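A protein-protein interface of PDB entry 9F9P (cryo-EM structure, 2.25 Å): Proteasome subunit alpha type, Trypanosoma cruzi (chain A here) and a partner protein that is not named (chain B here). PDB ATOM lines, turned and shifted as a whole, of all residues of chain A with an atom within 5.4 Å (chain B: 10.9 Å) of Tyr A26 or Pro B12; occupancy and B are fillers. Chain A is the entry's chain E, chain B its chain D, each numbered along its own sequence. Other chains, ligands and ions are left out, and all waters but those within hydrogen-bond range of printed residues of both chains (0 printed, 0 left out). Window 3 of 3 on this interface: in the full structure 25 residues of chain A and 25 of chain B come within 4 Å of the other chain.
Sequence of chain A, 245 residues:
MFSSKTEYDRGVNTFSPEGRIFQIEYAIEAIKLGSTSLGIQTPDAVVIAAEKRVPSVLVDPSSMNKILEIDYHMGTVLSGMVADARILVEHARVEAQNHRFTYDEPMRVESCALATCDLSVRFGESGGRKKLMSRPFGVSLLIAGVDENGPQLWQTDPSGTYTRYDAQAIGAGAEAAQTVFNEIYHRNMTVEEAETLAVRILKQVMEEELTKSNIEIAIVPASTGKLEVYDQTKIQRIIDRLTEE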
ATOM      1  N   ARG A  10      17.428 -11.186  -9.426  1.00  0.00           N
ATOM      2  CA  ARG A  10      17.560 -11.918 -10.677  1.00  0.00           C
ATOM      3  C   ARG A  10      18.473 -11.148 -11.638  1.00  0.00           C
ATOM      4  O   ARG A  10      18.316  -9.951 -11.845  1.00  0.00           O
ATOM      5  CB  ARG A  10      16.187 -12.200 -11.284  1.00  0.00           C
ATOM      6  CG  ARG A  10      15.513 -10.993 -11.910  1.00  0.00           C
ATOM      7  CD  ARG A  10      14.313 -11.468 -12.685  1.00  0.00           C
ATOM      8  NE  ARG A  10      13.141 -11.841 -11.907  1.00  0.00           N
ATOM      9  CZ  ARG A  10      11.987 -11.179 -11.968  1.00  0.00           C
ATOM     10  NH1 ARG A  10      11.967  -9.931 -12.411  1.00  0.00           N
ATOM     11  NH2 ARG A  10      10.869 -11.750 -11.550  1.00  0.00           N
ATOM     12  N   PHE A  22      14.557  -9.019 -19.293  1.00  0.00           N
ATOM     13  CA  PHE A  22      13.983  -8.029 -18.377  1.00  0.00           C
ATOM     14  C   PHE A  22      14.669  -6.652 -18.429  1.00  0.00           C
ATOM     15  O   PHE A  22      14.012  -5.639 -18.488  1.00  0.00           O
ATOM     16  CB  PHE A  22      14.088  -8.558 -16.946  1.00  0.00           C
ATOM     17  CG  PHE A  22      13.053  -9.586 -16.539  1.00  0.00           C
ATOM     18  CD1 PHE A  22      11.689  -9.275 -16.555  1.00  0.00           C
ATOM     19  CD2 PHE A  22      13.444 -10.845 -16.086  1.00  0.00           C
ATOM     20  CE1 PHE A  22      10.741 -10.206 -16.152  1.00  0.00           C
ATOM     21  CE2 PHE A  22      12.498 -11.781 -15.680  1.00  0.00           C
ATOM     22  CZ  PHE A  22      11.148 -11.458 -15.710  1.00  0.00           C
ATOM     23  N   GLN A  23      15.998  -6.601 -18.389  1.00  0.00           N
ATOM     24  CA  GLN A  23      16.692  -5.324 -18.409  1.00  0.00           C
ATOM     25  C   GLN A  23      16.410  -4.529 -19.685  1.00  0.00           C
ATOM     26  O   GLN A  23      16.516  -3.312 -19.682  1.00  0.00           O
ATOM     27  CB  GLN A  23      18.210  -5.499 -18.379  1.00  0.00           C
ATOM     28  CG  GLN A  23      18.794  -5.895 -17.030  1.00  0.00           C
ATOM     29  CD  GLN A  23      18.584  -4.835 -15.977  1.00  0.00           C
ATOM     30  OE1 GLN A  23      19.255  -3.809 -15.956  1.00  0.00           O
ATOM     31  NE2 GLN A  23      17.643  -5.096 -15.092  1.00  0.00           N
ATOM     32  N   ILE A  24      16.133  -5.207 -20.800  1.00  0.00           N
ATOM     33  CA  ILE A  24      15.805  -4.522 -22.041  1.00  0.00           C
ATOM     34  C   ILE A  24      14.384  -3.983 -21.991  1.00  0.00           C
ATOM     35  O   ILE A  24      14.159  -2.880 -22.444  1.00  0.00           O
ATOM     36  CB  ILE A  24      16.092  -5.417 -23.252  1.00  0.00           C
ATOM     37  CG1 ILE A  24      17.603  -5.538 -23.444  1.00  0.00           C
ATOM     38  CG2 ILE A  24      15.429  -4.868 -24.496  1.00  0.00           C
ATOM     39  CD1 ILE A  24      18.025  -6.563 -24.472  1.00  0.00           C
ATOM     40  N   GLU A  25      13.462  -4.660 -21.324  1.00  0.00           N
ATOM     41  CA  GLU A  25      12.102  -4.161 -21.205  1.00  0.00           C
ATOM     42  C   GLU A  25      12.045  -2.923 -20.321  1.00  0.00           C
ATOM     43  O   GLU A  25      11.330  -1.971 -20.609  1.00  0.00           O
ATOM     44  CB  GLU A  25      11.203  -5.265 -20.665  1.00  0.00           C
ATOM     45  CG  GLU A  25      11.111  -6.447 -21.637  1.00  0.00           C
ATOM     46  CD  GLU A  25      10.477  -6.127 -23.001  1.00  0.00           C
ATOM     47  OE1 GLU A  25       9.234  -5.920 -23.043  1.00  0.00           O
ATOM     48  OE2 GLU A  25      11.220  -6.065 -24.033  1.00  0.00           O
ATOM     49  N   TYR A  26      12.841  -2.908 -19.271  1.00  0.00           N
ATOM     50  CA  TYR A  26      12.868  -1.779 -18.361  1.00  0.00           C
ATOM     51  C   TYR A  26      13.549  -0.569 -19.001  1.00  0.00           C
ATOM     52  O   TYR A  26      13.121   0.565 -18.830  1.00  0.00           O
ATOM     53  CB  TYR A  26      13.609  -2.200 -17.090  1.00  0.00           C
ATOM     54  CG  TYR A  26      13.043  -3.379 -16.330  1.00  0.00           C
ATOM     55  CD1 TYR A  26      11.721  -3.771 -16.444  1.00  0.00           C
ATOM     56  CD2 TYR A  26      13.855  -4.104 -15.462  1.00  0.00           C
ATOM     57  CE1 TYR A  26      11.226  -4.841 -15.716  1.00  0.00           C
ATOM     58  CE2 TYR A  26      13.368  -5.176 -14.713  1.00  0.00           C
ATOM     59  CZ  TYR A  26      12.047  -5.544 -14.838  1.00  0.00           C
ATOM     60  OH  TYR A  26      11.597  -6.618 -14.101  1.00  0.00           O
ATOM     61  N   ALA A  27      14.651  -0.788 -19.713  1.00  0.00           N
ATOM     62  CA  ALA A  27      15.268   0.304 -20.453  1.00  0.00           C
ATOM     63  C   ALA A  27      14.281   0.971 -21.406  1.00  0.00           C
ATOM     64  O   ALA A  27      14.262   2.188 -21.495  1.00  0.00           O
ATOM     65  CB  ALA A  27      16.480  -0.194 -21.189  1.00  0.00           C
ATOM     66  N   ILE A  28      13.390   0.210 -22.044  1.00  0.00           N
ATOM     67  CA  ILE A  28      12.373   0.775 -22.924  1.00  0.00           C
ATOM     68  C   ILE A  28      11.339   1.571 -22.145  1.00  0.00           C
ATOM     69  O   ILE A  28      10.804   2.532 -22.672  1.00  0.00           O
ATOM     70  CB  ILE A  28      11.731  -0.330 -23.805  1.00  0.00           C
ATOM     71  CG1 ILE A  28      12.732  -0.790 -24.869  1.00  0.00           C
ATOM     72  CG2 ILE A  28      10.417   0.099 -24.457  1.00  0.00           C
ATOM     73  CD1 ILE A  28      12.420  -2.131 -25.429  1.00  0.00           C
ATOM     74  N   GLU A  29      11.027   1.200 -20.911  1.00  0.00           N
ATOM     75  CA  GLU A  29      10.168   2.051 -20.085  1.00  0.00           C
ATOM     76  C   GLU A  29      10.809   3.408 -19.774  1.00  0.00           C
ATOM     77  O   GLU A  29      10.121   4.414 -19.674  1.00  0.00           O
ATOM     78  CB  GLU A  29       9.818   1.354 -18.769  1.00  0.00           C
ATOM     79  CG  GLU A  29       8.649   0.403 -18.891  1.00  0.00           C
ATOM     80  CD  GLU A  29       7.396   1.072 -19.457  1.00  0.00           C
ATOM     81  OE1 GLU A  29       6.730   0.461 -20.348  1.00  0.00           O
ATOM     82  OE2 GLU A  29       7.103   2.230 -19.036  1.00  0.00           O
ATOM     83  N   ALA A  30      12.123   3.460 -19.591  1.00  0.00           N
ATOM     84  CA  ALA A  30      12.780   4.701 -19.216  1.00  0.00           C
ATOM     85  C   ALA A  30      12.724   5.727 -20.348  1.00  0.00           C
ATOM     86  O   ALA A  30      12.786   6.923 -20.102  1.00  0.00           O
ATOM     87  CB  ALA A  30      14.210   4.423 -18.825  1.00  0.00           C
ATOM     88  N   THR B   8      24.839  -1.128 -10.780  1.00  0.00           N
ATOM     89  CA  THR B   8      23.823  -0.201 -11.269  1.00  0.00           C
ATOM     90  C   THR B   8      22.954  -0.858 -12.358  1.00  0.00           C
ATOM     91  O   THR B   8      23.413  -1.064 -13.472  1.00  0.00           O
ATOM     92  CB  THR B   8      24.515   1.071 -11.809  1.00  0.00           C
ATOM     93  OG1 THR B   8      25.462   1.673 -10.921  1.00  0.00           O
ATOM     94  CG2 THR B   8      23.522   2.144 -12.167  1.00  0.00           C
ATOM     95  N   VAL B   9      21.701  -1.201 -12.052  1.00  0.00           N
ATOM     96  CA  VAL B   9      20.849  -1.890 -13.014  1.00  0.00           C
ATOM     97  C   VAL B   9      19.494  -1.202 -13.075  1.00  0.00           C
ATOM     98  O   VAL B   9      19.092  -0.544 -12.122  1.00  0.00           O
ATOM     99  CB  VAL B   9      20.679  -3.389 -12.661  1.00  0.00           C
ATOM    100  CG1 VAL B   9      21.994  -4.139 -12.768  1.00  0.00           C
ATOM    101  CG2 VAL B   9      20.076  -3.602 -11.281  1.00  0.00           C
ATOM    102  N   PHE B  10      18.762  -1.417 -14.169  1.00  0.00           N
ATOM    103  CA  PHE B  10      17.402  -0.917 -14.258  1.00  0.00           C
ATOM    104  C   PHE B  10      16.521  -1.772 -13.386  1.00  0.00           C
ATOM    105  O   PHE B  10      16.751  -2.966 -13.263  1.00  0.00           O
ATOM    106  CB  PHE B  10      16.787  -0.978 -15.663  1.00  0.00           C
ATOM    107  CG  PHE B  10      17.325   0.025 -16.628  1.00  0.00           C
ATOM    108  CD1 PHE B  10      16.846   1.316 -16.635  1.00  0.00           C
ATOM    109  CD2 PHE B  10      18.363  -0.296 -17.468  1.00  0.00           C
ATOM    110  CE1 PHE B  10      17.388   2.280 -17.478  1.00  0.00           C
ATOM    111  CE2 PHE B  10      18.895   0.665 -18.333  1.00  0.00           C
ATOM    112  CZ  PHE B  10      18.438   1.960 -18.309  1.00  0.00           C
ATOM    113  N   SER B  11      15.485  -1.133 -12.862  1.00  0.00           N
ATOM    114  CA  SER B  11      14.401  -1.788 -12.150  1.00  0.00           C
ATOM    115  C   SER B  11      13.089  -1.527 -12.896  1.00  0.00           C
ATOM    116  O   SER B  11      13.056  -0.664 -13.759  1.00  0.00           O
ATOM    117  CB  SER B  11      14.342  -1.231 -10.768  1.00  0.00           C
ATOM    118  OG  SER B  11      13.825   0.087 -10.881  1.00  0.00           O
ATOM    119  N   PRO B  12      11.981  -2.240 -12.562  1.00  0.00           N
ATOM    120  CA  PRO B  12      10.727  -2.198 -13.325  1.00  0.00           C
ATOM    121  C   PRO B  12       9.994  -0.953 -13.825  1.00  0.00           C
ATOM    122  O   PRO B  12       9.156  -1.092 -14.715  1.00  0.00           O
ATOM    123  CB  PRO B  12       9.755  -2.904 -12.362  1.00  0.00           C
ATOM    124  CG  PRO B  12      10.603  -3.997 -11.769  1.00  0.00           C
ATOM    125  CD  PRO B  12      11.942  -3.317 -11.549  1.00  0.00           C
ATOM    126  N   ASP B  13      10.252   0.261 -13.366  1.00  0.00           N
ATOM    127  CA  ASP B  13       9.558   1.345 -14.067  1.00  0.00           C
ATOM    128  C   ASP B  13      10.528   2.272 -14.802  1.00  0.00           C
ATOM    129  O   ASP B  13      10.198   3.433 -15.036  1.00  0.00           O
ATOM    130  CB  ASP B  13       8.641   2.134 -13.123  1.00  0.00           C
ATOM    131  CG  ASP B  13       7.455   1.328 -12.604  1.00  0.00           C
ATOM    132  OD1 ASP B  13       6.755   0.698 -13.437  1.00  0.00           O
ATOM    133  OD2 ASP B  13       7.220   1.348 -11.367  1.00  0.00           O
ATOM    134  N   GLY B  14      11.713   1.764 -15.153  1.00  0.00           N
ATOM    135  CA  GLY B  14      12.766   2.563 -15.766  1.00  0.00           C
ATOM    136  C   GLY B  14      13.705   3.288 -14.784  1.00  0.00           C
ATOM    137  O   GLY B  14      14.501   4.115 -15.205  1.00  0.00           O
ATOM    138  N   HIS B  15      13.668   2.968 -13.493  1.00  0.00           N
ATOM    139  CA  HIS B  15      14.513   3.658 -12.524  1.00  0.00           C
ATOM    140  C   HIS B  15      15.913   3.039 -12.488  1.00  0.00           C
ATOM    141  O   HIS B  15      16.053   1.836 -12.707  1.00  0.00           O
ATOM    142  CB  HIS B  15      13.815   3.663 -11.155  1.00  0.00           C
ATOM    143  CG  HIS B  15      12.537   4.443 -11.182  1.00  0.00           C
ATOM    144  ND1 HIS B  15      11.316   3.900 -10.835  1.00  0.00           N
ATOM    145  CD2 HIS B  15      12.295   5.713 -11.570  1.00  0.00           C
ATOM    146  CE1 HIS B  15      10.377   4.823 -10.991  1.00  0.00           C
ATOM    147  NE2 HIS B  15      10.949   5.930 -11.443  1.00  0.00           N
ATOM    148  N   LEU B  16      16.938   3.868 -12.272  1.00  0.00           N
ATOM    149  CA  LEU B  16      18.238   3.377 -11.835  1.00  0.00           C
ATOM    150  C   LEU B  16      18.480   3.774 -10.377  1.00  0.00           C
ATOM    151  O   LEU B  16      18.950   4.884 -10.123  1.00  0.00           O
ATOM    152  CB  LEU B  16      19.356   3.974 -12.692  1.00  0.00           C
ATOM    153  CG  LEU B  16      19.351   3.620 -14.172  1.00  0.00           C
ATOM    154  CD1 LEU B  16      20.386   4.440 -14.933  1.00  0.00           C
ATOM    155  CD2 LEU B  16      19.666   2.139 -14.357  1.00  0.00           C
ATOM    156  N   PHE B  17      18.246   2.852  -9.446  1.00  0.00           N
ATOM    157  CA  PHE B  17      18.225   3.180  -8.033  1.00  0.00           C
ATOM    158  C   PHE B  17      19.592   3.628  -7.537  1.00  0.00           C
ATOM    159  O   PHE B  17      19.679   4.589  -6.785  1.00  0.00           O
ATOM    160  CB  PHE B  17      17.777   1.992  -7.182  1.00  0.00           C
ATOM    161  CG  PHE B  17      16.305   1.684  -7.205  1.00  0.00           C
ATOM    162  CD1 PHE B  17      15.356   2.695  -7.280  1.00  0.00           C
ATOM    163  CD2 PHE B  17      15.867   0.368  -7.098  1.00  0.00           C
ATOM    164  CE1 PHE B  17      14.002   2.394  -7.293  1.00  0.00           C
ATOM    165  CE2 PHE B  17      14.509   0.073  -7.101  1.00  0.00           C
ATOM    166  CZ  PHE B  17      13.581   1.085  -7.201  1.00  0.00           C
ATOM    167  N   GLU B  20      19.724   7.329  -8.275  1.00  0.00           N
ATOM    168  CA  GLU B  20      18.880   8.169  -7.429  1.00  0.00           C
ATOM    169  C   GLU B  20      19.376   8.258  -5.983  1.00  0.00           C
ATOM    170  O   GLU B  20      19.207   9.268  -5.331  1.00  0.00           O
ATOM    171  CB  GLU B  20      17.459   7.610  -7.384  1.00  0.00           C
ATOM    172  CG  GLU B  20      16.810   7.576  -8.761  1.00  0.00           C
ATOM    173  CD  GLU B  20      15.509   6.792  -8.903  1.00  0.00           C
ATOM    174  OE1 GLU B  20      15.144   6.023  -7.957  1.00  0.00           O
ATOM    175  OE2 GLU B  20      14.854   6.942  -9.970  1.00  0.00           O
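Arg A10 touches none of the printed residues of chain B.
No residue of chain B comes within 4 Å of Glu A25.
Tyr A26 touches just these residues of chain B: Phe B10, Ser B11, Pro B12 and Gly B14.
Ala A27 touches one residue of chain B.
No residue of chain B comes within 4 Å of Ile A28.
Of the printed residues of chain A, Val B9 touches Gln A23 (3.6 Å).
Of the printed residues of chain A, Phe B10 touches Gln A23, Tyr A26 and Ala A27.
Printed residues of chain A within 4 Å of Ser B11: Tyr A26 (3.7 Å).
Of the printed residues of chain A, Pro B12 touches Tyr A26 (3.6 Å).
Asp B13 touches none of the printed residues of chain A.
Of the printed residues of chain A, Gly B14 touches Tyr A26 (3.7 Å) and Ala A30 (3.6 Å).
Hydrophobic or aromatic side chains of chain A that line the printed part of chain B: Tyr A26, Ala A27 and Ala A30.
Among the printed residues, 8 pairs touch across the chains.
The side-chain hydroxyl (OG) of Ser B11 lies within hydrogen-bond range of the backbone carbonyl oxygen (O) of His B15 (3.4 Å).
O of Phe B10 is in hydrogen-bond range of NE2 of Gln A23.
Gln A23 touches Val B9 (OE1 to CB, 3.6 Å).
CB of Phe B10 touches CB of Tyr A26, at 3.7 Å.
O of Ser B11 touches CB of Tyr A26 (3.7 Å).
Tyr A26 touches Pro B12.
Tyr A26 touches Gly B14.
CE2 of Phe B10 touches CB of Ala A27, 3.8 Å away.
Ala A30 touches Gly B14.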
